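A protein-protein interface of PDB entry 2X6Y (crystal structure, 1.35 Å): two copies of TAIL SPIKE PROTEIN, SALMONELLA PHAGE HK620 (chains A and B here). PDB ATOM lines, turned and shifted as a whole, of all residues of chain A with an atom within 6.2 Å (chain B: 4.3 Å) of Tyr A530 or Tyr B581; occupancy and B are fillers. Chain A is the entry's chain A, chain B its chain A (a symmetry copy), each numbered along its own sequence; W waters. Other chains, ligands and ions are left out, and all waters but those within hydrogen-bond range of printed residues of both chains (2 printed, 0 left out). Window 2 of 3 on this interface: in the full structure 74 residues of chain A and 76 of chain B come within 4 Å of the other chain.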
ATOM      1  N   THR A 528      22.352  -4.171 -18.493  1.00  0.00           N
ATOM      2  CA  THR A 528      21.423  -5.272 -18.217  1.00  0.00           C
ATOM      3  C   THR A 528      21.916  -6.507 -18.980  1.00  0.00           C
ATOM      4  O   THR A 528      22.421  -6.401 -20.085  1.00  0.00           O
ATOM      5  CB  THR A 528      19.987  -4.889 -18.621  1.00  0.00           C
ATOM      6  OG1 THR A 528      19.568  -3.772 -17.822  1.00  0.00           O
ATOM      7  CG2 THR A 528      19.011  -6.043 -18.447  1.00  0.00           C
ATOM      8  N   SER A 529      21.789  -7.684 -18.380  1.00  0.00           N
ATOM      9  CA  SER A 529      22.145  -8.932 -19.022  1.00  0.00           C
ATOM     10  C   SER A 529      20.950  -9.695 -19.544  1.00  0.00           C
ATOM     11  O   SER A 529      19.803  -9.428 -19.147  1.00  0.00           O
ATOM     12  CB  SER A 529      22.887  -9.820 -18.043  1.00  0.00           C
ATOM     13  OG  SER A 529      22.004 -10.484 -17.143  1.00  0.00           O
ATOM     14  N   TYR A 530      21.225 -10.647 -20.428  1.00  0.00           N
ATOM     15  CA  TYR A 530      20.286 -11.691 -20.719  1.00  0.00           C
ATOM     16  C   TYR A 530      20.129 -12.646 -19.538  1.00  0.00           C
ATOM     17  O   TYR A 530      20.895 -12.592 -18.572  1.00  0.00           O
ATOM     18  CB  TYR A 530      20.681 -12.453 -21.989  1.00  0.00           C
ATOM     19  CG  TYR A 530      20.590 -11.672 -23.298  1.00  0.00           C
ATOM     20  CD1 TYR A 530      19.904 -10.460 -23.389  1.00  0.00           C
ATOM     21  CD2 TYR A 530      21.163 -12.178 -24.464  1.00  0.00           C
ATOM     22  CE1 TYR A 530      19.817  -9.775 -24.607  1.00  0.00           C
ATOM     23  CE2 TYR A 530      21.078 -11.507 -25.662  1.00  0.00           C
ATOM     24  CZ  TYR A 530      20.405 -10.305 -25.737  1.00  0.00           C
ATOM     25  OH  TYR A 530      20.326  -9.637 -26.938  1.00  0.00           O
ATOM     26  N   ASN A 531      19.112 -13.498 -19.612  1.00  0.00           N
ATOM     27  CA  ASN A 531      18.753 -14.409 -18.506  1.00  0.00           C
ATOM     28  C   ASN A 531      19.662 -15.634 -18.357  1.00  0.00           C
ATOM     29  O   ASN A 531      19.736 -16.254 -17.295  1.00  0.00           O
ATOM     30  CB  ASN A 531      17.305 -14.882 -18.742  1.00  0.00           C
ATOM     31  CG  ASN A 531      16.848 -15.907 -17.747  1.00  0.00           C
ATOM     32  OD1 ASN A 531      16.747 -15.624 -16.558  1.00  0.00           O
ATOM     33  ND2 ASN A 531      16.565 -17.115 -18.224  1.00  0.00           N
ATOM     34  N   THR A 532      20.360 -15.974 -19.422  1.00  0.00           N
ATOM     35  CA  THR A 532      20.986 -17.288 -19.540  1.00  0.00           C
ATOM     36  C   THR A 532      21.998 -17.562 -18.424  1.00  0.00           C
ATOM     37  O   THR A 532      22.782 -16.700 -18.046  1.00  0.00           O
ATOM     38  CB  THR A 532      21.697 -17.428 -20.916  1.00  0.00           C
ATOM     39  OG1 THR A 532      21.117 -16.519 -21.870  1.00  0.00           O
ATOM     40  CG2 THR A 532      21.582 -18.864 -21.443  1.00  0.00           C
ATOM     41  N   ALA A 535      28.059 -18.239 -19.342  1.00  0.00           N
ATOM     42  CA  ALA A 535      28.594 -17.072 -20.038  1.00  0.00           C
ATOM     43  C   ALA A 535      27.421 -16.306 -20.653  1.00  0.00           C
ATOM     44  O   ALA A 535      26.596 -16.895 -21.383  1.00  0.00           O
ATOM     45  CB  ALA A 535      29.629 -17.473 -21.127  1.00  0.00           C
ATOM     46  N   VAL A 536      27.321 -15.015 -20.350  1.00  0.00           N
ATOM     47  CA  VAL A 536      26.114 -14.265 -20.653  1.00  0.00           C
ATOM     48  C   VAL A 536      26.470 -12.818 -20.974  1.00  0.00           C
ATOM     49  O   VAL A 536      27.336 -12.226 -20.317  1.00  0.00           O
ATOM     50  CB  VAL A 536      25.084 -14.344 -19.457  1.00  0.00           C
ATOM     51  CG1 VAL A 536      25.643 -13.683 -18.205  1.00  0.00           C
ATOM     52  CG2 VAL A 536      23.745 -13.723 -19.839  1.00  0.00           C
ATOM     53  N   PRO A 537      25.833 -12.244 -22.005  1.00  0.00           N
ATOM     54  CA  PRO A 537      26.163 -10.884 -22.371  1.00  0.00           C
ATOM     55  C   PRO A 537      25.477  -9.865 -21.496  1.00  0.00           C
ATOM     56  O   PRO A 537      24.359 -10.094 -21.043  1.00  0.00           O
ATOM     57  CB  PRO A 537      25.676 -10.791 -23.816  1.00  0.00           C
ATOM     58  CG  PRO A 537      24.490 -11.676 -23.819  1.00  0.00           C
ATOM     59  CD  PRO A 537      24.905 -12.858 -22.982  1.00  0.00           C
ATOM     60  N   PHE A 538      26.183  -8.770 -21.264  1.00  0.00           N
ATOM     61  CA  PHE A 538      25.653  -7.570 -20.642  1.00  0.00           C
ATOM     62  C   PHE A 538      25.728  -6.442 -21.679  1.00  0.00           C
ATOM     63  O   PHE A 538      26.735  -6.314 -22.373  1.00  0.00           O
ATOM     64  CB  PHE A 538      26.496  -7.167 -19.425  1.00  0.00           C
ATOM     65  CG  PHE A 538      26.271  -7.989 -18.199  1.00  0.00           C
ATOM     66  CD1 PHE A 538      26.619  -9.324 -18.158  1.00  0.00           C
ATOM     67  CD2 PHE A 538      25.734  -7.409 -17.042  1.00  0.00           C
ATOM     68  CE1 PHE A 538      26.426 -10.069 -16.983  1.00  0.00           C
ATOM     69  CE2 PHE A 538      25.545  -8.146 -15.871  1.00  0.00           C
ATOM     70  CZ  PHE A 538      25.888  -9.481 -15.841  1.00  0.00           C
ATOM     71  N   PHE A 539      24.689  -5.616 -21.717  1.00  0.00           N
ATOM     72  CA  PHE A 539      24.535  -4.537 -22.683  1.00  0.00           C
ATOM     73  C   PHE A 539      24.202  -3.224 -21.974  1.00  0.00           C
ATOM     74  O   PHE A 539      23.417  -3.208 -21.016  1.00  0.00           O
ATOM     75  CB  PHE A 539      23.378  -4.829 -23.646  1.00  0.00           C
ATOM     76  CG  PHE A 539      23.527  -6.101 -24.450  1.00  0.00           C
ATOM     77  CD1 PHE A 539      22.945  -7.280 -24.016  1.00  0.00           C
ATOM     78  CD2 PHE A 539      24.196  -6.096 -25.654  1.00  0.00           C
ATOM     79  CE1 PHE A 539      23.065  -8.433 -24.749  1.00  0.00           C
ATOM     80  CE2 PHE A 539      24.313  -7.249 -26.395  1.00  0.00           C
ATOM     81  CZ  PHE A 539      23.740  -8.418 -25.932  1.00  0.00           C
ATOM     82  N   LYS A 571      28.712  -1.987 -30.089  1.00  0.00           N
ATOM     83  CA  LYS A 571      27.875  -2.460 -31.187  1.00  0.00           C
ATOM     84  C   LYS A 571      27.494  -1.271 -32.053  1.00  0.00           C
ATOM     85  O   LYS A 571      27.561  -0.114 -31.621  1.00  0.00           O
ATOM     86  CB  LYS A 571      26.556  -3.026 -30.637  1.00  0.00           C
ATOM     87  CG  LYS A 571      26.675  -4.314 -29.886  1.00  0.00           C
ATOM     88  CD  LYS A 571      25.376  -4.703 -29.162  1.00  0.00           C
ATOM     89  CE  LYS A 571      24.148  -4.660 -30.042  1.00  0.00           C
ATOM     90  NZ  LYS A 571      22.963  -5.269 -29.355  1.00  0.00           N
ATOM     91  N   VAL A 577      28.825  -3.758 -25.052  1.00  0.00           N
ATOM     92  CA  VAL A 577      28.537  -5.181 -24.855  1.00  0.00           C
ATOM     93  C   VAL A 577      29.775  -5.887 -24.335  1.00  0.00           C
ATOM     94  O   VAL A 577      30.897  -5.587 -24.737  1.00  0.00           O
ATOM     95  CB  VAL A 577      28.066  -5.866 -26.160  1.00  0.00           C
ATOM     96  CG1 VAL A 577      29.077  -5.691 -27.276  1.00  0.00           C
ATOM     97  CG2 VAL A 577      27.757  -7.362 -25.933  1.00  0.00           C
ATOM     98  N   GLY A 578      29.572  -6.794 -23.383  1.00  0.00           N
ATOM     99  CA  GLY A 578      30.647  -7.656 -22.932  1.00  0.00           C
ATOM    100  C   GLY A 578      30.095  -8.959 -22.419  1.00  0.00           C
ATOM    101  O   GLY A 578      28.886  -9.080 -22.215  1.00  0.00           O
ATOM    102  N   VAL A 579      30.970  -9.939 -22.191  1.00  0.00           N
ATOM    103  CA  VAL A 579      30.555 -11.268 -21.726  1.00  0.00           C
ATOM    104  C   VAL A 579      30.921 -11.444 -20.240  1.00  0.00           C
ATOM    105  O   VAL A 579      32.101 -11.417 -19.863  1.00  0.00           O
ATOM    106  CB  VAL A 579      31.186 -12.407 -22.584  1.00  0.00           C
ATOM    107  CG1 VAL A 579      30.785 -13.759 -22.053  1.00  0.00           C
ATOM    108  CG2 VAL A 579      30.755 -12.278 -24.022  1.00  0.00           C
ATOM    109  N   ASN A 582      26.925 -15.770 -15.325  1.00  0.00           N
ATOM    110  CA  ASN A 582      25.796 -16.028 -14.424  1.00  0.00           C
ATOM    111  C   ASN A 582      26.005 -17.407 -13.790  1.00  0.00           C
ATOM    112  O   ASN A 582      25.809 -18.437 -14.444  1.00  0.00           O
ATOM    113  CB  ASN A 582      24.472 -16.051 -15.214  1.00  0.00           C
ATOM    114  CG  ASN A 582      23.599 -14.821 -15.005  1.00  0.00           C
ATOM    115  OD1 ASN A 582      23.762 -14.057 -14.044  1.00  0.00           O
ATOM    116  ND2 ASN A 582      22.627 -14.645 -15.905  1.00  0.00           N
ATOM    117  N   GLY A 586      19.315 -15.609 -14.585  1.00  0.00           N
ATOM    118  CA  GLY A 586      18.527 -14.444 -14.253  1.00  0.00           C
ATOM    119  C   GLY A 586      18.992 -13.193 -14.971  1.00  0.00           C
ATOM    120  O   GLY A 586      20.190 -13.007 -15.180  1.00  0.00           O
ATOM    121  N   VAL A 587      18.037 -12.349 -15.357  1.00  0.00           N
ATOM    122  CA  VAL A 587      18.335 -11.015 -15.866  1.00  0.00           C
ATOM    123  C   VAL A 587      19.001 -10.211 -14.758  1.00  0.00           C
ATOM    124  O   VAL A 587      18.484 -10.154 -13.629  1.00  0.00           O
ATOM    125  CB  VAL A 587      17.074 -10.313 -16.353  1.00  0.00           C
ATOM    126  CG1 VAL A 587      17.365  -8.878 -16.692  1.00  0.00           C
ATOM    127  CG2 VAL A 587      16.506 -11.064 -17.576  1.00  0.00           C
ATOM    128  N   ARG A 588      20.146  -9.613 -15.076  1.00  0.00           N
ATOM    129  CA  ARG A 588      20.885  -8.775 -14.145  1.00  0.00           C
ATOM    130  C   ARG A 588      20.858  -7.327 -14.585  1.00  0.00           C
ATOM    131  O   ARG A 588      20.787  -7.045 -15.785  1.00  0.00           O
ATOM    132  CB  ARG A 588      22.336  -9.241 -14.032  1.00  0.00           C
ATOM    133  CG  ARG A 588      22.520 -10.722 -13.807  1.00  0.00           C
ATOM    134  CD  ARG A 588      21.809 -11.207 -12.567  1.00  0.00           C
ATOM    135  NE  ARG A 588      22.119 -12.608 -12.325  1.00  0.00           N
ATOM    136  CZ  ARG A 588      21.839 -13.246 -11.198  1.00  0.00           C
ATOM    137  NH1 ARG A 588      21.222 -12.625 -10.184  1.00  0.00           N
ATOM    138  NH2 ARG A 588      22.177 -14.517 -11.069  1.00  0.00           N
ATOM    139  N   GLN B 533      26.160 -19.628 -31.935  1.00  0.00           N
ATOM    140  CA  GLN B 533      25.403 -18.534 -31.338  1.00  0.00           C
ATOM    141  C   GLN B 533      25.775 -18.404 -29.863  1.00  0.00           C
ATOM    142  O   GLN B 533      26.047 -19.408 -29.190  1.00  0.00           O
ATOM    143  CB  GLN B 533      23.898 -18.770 -31.505  1.00  0.00           C
ATOM    144  CG  GLN B 533      23.029 -17.560 -31.160  1.00  0.00           C
ATOM    145  CD  GLN B 533      22.768 -17.370 -29.676  1.00  0.00           C
ATOM    146  OE1 GLN B 533      22.800 -18.323 -28.878  1.00  0.00           O
ATOM    147  NE2 GLN B 533      22.531 -16.125 -29.288  1.00  0.00           N
ATOM    148  N   GLY B 534      25.816 -17.164 -29.392  1.00  0.00           N
ATOM    149  CA  GLY B 534      26.120 -16.855 -28.004  1.00  0.00           C
ATOM    150  C   GLY B 534      27.590 -16.546 -27.814  1.00  0.00           C
ATOM    151  O   GLY B 534      28.247 -16.032 -28.702  1.00  0.00           O
ATOM    152  N   ALA B 535      28.114 -16.844 -26.630  1.00  0.00           N
ATOM    153  CA  ALA B 535      29.529 -16.631 -26.340  1.00  0.00           C
ATOM    154  C   ALA B 535      30.346 -17.516 -27.284  1.00  0.00           C
ATOM    155  O   ALA B 535      30.108 -18.740 -27.365  1.00  0.00           O
ATOM    156  CB  ALA B 535      29.866 -16.940 -24.853  1.00  0.00           C
ATOM    157  N   VAL B 536      31.283 -16.915 -28.011  1.00  0.00           N
ATOM    158  CA  VAL B 536      31.926 -17.600 -29.121  1.00  0.00           C
ATOM    159  C   VAL B 536      33.367 -17.126 -29.257  1.00  0.00           C
ATOM    160  O   VAL B 536      33.649 -15.930 -29.110  1.00  0.00           O
ATOM    161  CB  VAL B 536      31.125 -17.374 -30.463  1.00  0.00           C
ATOM    162  CG1 VAL B 536      31.127 -15.905 -30.865  1.00  0.00           C
ATOM    163  CG2 VAL B 536      31.680 -18.239 -31.590  1.00  0.00           C
ATOM    164  N   PHE B 562      26.879  -9.178 -33.889  1.00  0.00           N
ATOM    165  CA  PHE B 562      27.943  -9.795 -33.116  1.00  0.00           C
ATOM    166  C   PHE B 562      28.922  -8.741 -32.646  1.00  0.00           C
ATOM    167  O   PHE B 562      28.928  -7.597 -33.133  1.00  0.00           O
ATOM    168  CB  PHE B 562      28.695 -10.891 -33.888  1.00  0.00           C
ATOM    169  CG  PHE B 562      29.618 -10.374 -34.948  1.00  0.00           C
ATOM    170  CD1 PHE B 562      29.158 -10.098 -36.238  1.00  0.00           C
ATOM    171  CD2 PHE B 562      30.957 -10.166 -34.672  1.00  0.00           C
ATOM    172  CE1 PHE B 562      30.027  -9.634 -37.214  1.00  0.00           C
ATOM    173  CE2 PHE B 562      31.837  -9.720 -35.669  1.00  0.00           C
ATOM    174  CZ  PHE B 562      31.371  -9.449 -36.926  1.00  0.00           C
ATOM    175  N   SER B 563      29.794  -9.178 -31.753  1.00  0.00           N
ATOM    176  CA  SER B 563      30.925  -8.377 -31.325  1.00  0.00           C
ATOM    177  C   SER B 563      32.140  -9.284 -31.151  1.00  0.00           C
ATOM    178  O   SER B 563      32.021 -10.394 -30.637  1.00  0.00           O
ATOM    179  CB  SER B 563      30.612  -7.618 -30.035  1.00  0.00           C
ATOM    180  OG  SER B 563      30.196  -8.491 -28.999  1.00  0.00           O
ATOM    181  N   GLY B 580      34.087 -13.521 -27.775  1.00  0.00           N
ATOM    182  CA  GLY B 580      33.142 -12.519 -28.218  1.00  0.00           C
ATOM    183  C   GLY B 580      31.724 -13.038 -28.092  1.00  0.00           C
ATOM    184  O   GLY B 580      31.448 -14.009 -27.376  1.00  0.00           O
ATOM    185  N   TYR B 581      30.793 -12.377 -28.773  1.00  0.00           N
ATOM    186  CA  TYR B 581      29.390 -12.730 -28.624  1.00  0.00           C
ATOM    187  C   TYR B 581      28.654 -12.647 -29.969  1.00  0.00           C
ATOM    188  O   TYR B 581      28.606 -11.587 -30.592  1.00  0.00           O
ATOM    189  CB  TYR B 581      28.695 -11.829 -27.582  1.00  0.00           C
ATOM    190  CG  TYR B 581      27.312 -12.361 -27.247  1.00  0.00           C
ATOM    191  CD1 TYR B 581      27.170 -13.483 -26.447  1.00  0.00           C
ATOM    192  CD2 TYR B 581      26.160 -11.803 -27.808  1.00  0.00           C
ATOM    193  CE1 TYR B 581      25.929 -14.024 -26.170  1.00  0.00           C
ATOM    194  CE2 TYR B 581      24.910 -12.320 -27.521  1.00  0.00           C
ATOM    195  CZ  TYR B 581      24.801 -13.450 -26.715  1.00  0.00           C
ATOM    196  OH  TYR B 581      23.556 -14.005 -26.433  1.00  0.00           O
ATOM    197  N   ASN B 582      28.051 -13.763 -30.375  1.00  0.00           N
ATOM    198  CA  ASN B 582      27.234 -13.870 -31.589  1.00  0.00           C
ATOM    199  C   ASN B 582      25.762 -13.756 -31.178  1.00  0.00           C
ATOM    200  O   ASN B 582      25.189 -14.700 -30.624  1.00  0.00           O
ATOM    201  CB  ASN B 582      27.447 -15.243 -32.260  1.00  0.00           C
ATOM    202  CG  ASN B 582      28.283 -15.192 -33.533  1.00  0.00           C
ATOM    203  OD1 ASN B 582      28.469 -14.136 -34.152  1.00  0.00           O
ATOM    204  ND2 ASN B 582      28.765 -16.366 -33.951  1.00  0.00           N
ATOM    205  N   GLU B 583      25.125 -12.607 -31.427  1.00  0.00           N
ATOM    206  CA  GLU B 583      23.696 -12.472 -31.101  1.00  0.00           C
ATOM    207  C   GLU B 583      22.935 -13.481 -31.956  1.00  0.00           C
ATOM    208  O   GLU B 583      22.027 -14.175 -31.473  1.00  0.00           O
ATOM    209  CB  GLU B 583      23.195 -11.041 -31.313  1.00  0.00           C
ATOM    210  CG  GLU B 583      21.689 -10.870 -31.155  1.00  0.00           C
ATOM    211  CD  GLU B 583      21.210 -10.937 -29.711  1.00  0.00           C
ATOM    212  OE1 GLU B 583      21.975 -10.542 -28.807  1.00  0.00           O
ATOM    213  OE2 GLU B 583      20.045 -11.353 -29.489  1.00  0.00           O
HETATM  214  O   HOH W   1      23.220 -15.812 -24.264  1.00  0.00           O
HETATM  215  O   HOH W   2      23.243  -8.042 -29.580  1.00  0.00           O
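Water W2 bridges NZ of Lys A571 (2.8 Å) and OE1 of Glu B583 (2.9 Å).
Water W1 bridges the side-chain hydroxyl (OH) of Tyr B581 and the side-chain hydroxyl (OG1) of Thr A532.
OH of Tyr A530 lies within hydrogen-bond range of OE1 of Glu B583, 2.7 Å away.
O of Glu B583 lies within hydrogen-bond range of NE2 of Gln B533 (3.0 Å).
O of Val B536 sits at hydrogen-bond distance from N of Gly B580 (2.8 Å).
The backbone carbonyl oxygen of Thr A528 is in hydrogen-bond range of the backbone NH of Phe A539 (2.9 Å).
The backbone NH of Tyr A530 is in hydrogen-bond range of the backbone carbonyl oxygen of Pro A537, 3.2 Å away.
N of Ser B563 lies within hydrogen-bond range of O of Tyr B581, at 2.9 Å.
Of the 10 printed residues of chain B, 5 touch a printed residue of chain A.
Hydrophobic or aromatic side chains of chain B within 4 Å of the printed part of chain A: Ala B535 and Tyr B581.
Of the 18 printed residues of chain A, 6 touch a printed residue of chain B.
Hydrophobic or aromatic side chains of chain A that line the printed part of chain B: Tyr A530, Ala A535, Pro A537, Phe A539, Val A577 and Val A579.
Along chain A the printed residues that touch a printed residue of chain B span positions 530 to 579.
Among the printed residues, 7 pairs touch across the chains.
Among the printed residues, no Asp or Glu carboxylate lies within 4 Å of a Lys or Arg side-chain nitrogen of the other chain.
Tyr A530 touches just these residues of chain B: Tyr B581 (3.6 Å) and Glu B583 (2.7 Å).
Tyr B581 touches two residues of chain A.
Of the printed residues of chain A, Gly B580 touches Val A579.
Of the printed residues of chain A, Glu B583 touches Tyr A530 (2.7 Å) and Phe A539 (3.99 Å).
Printed residues of chain A within 4 Å of Ser B563: Val A577 (3.5 Å).
Printed residues of chain B within 4 Å of Val A577: Ser B563.
Of the printed residues of chain B, Ala A535 touches Ala B535.
The nearest printed residue of chain B that does not touch Tyr A530 is Gln B533 (6.0 Å).
The nearest printed residue of chain B that does not touch Pro A537 is Glu B583 (5.7 Å).
Ala B535 touches its own counterpart, Ala A535.
3 positions are printed for both chains.
Tyr A530 touches Tyr B581.
Ala A535 touches Ala B535 (CB to CB, 3.8 Å).
CZ of Tyr B581 touches CG of Pro A537 (3.4 Å).
Phe A539 touches Glu B583 (CZ to OE1, 3.99 Å).
Ser B563 touches Val A577.
O of Gly B580 touches CG2 of Val A579, 3.8 Å away.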
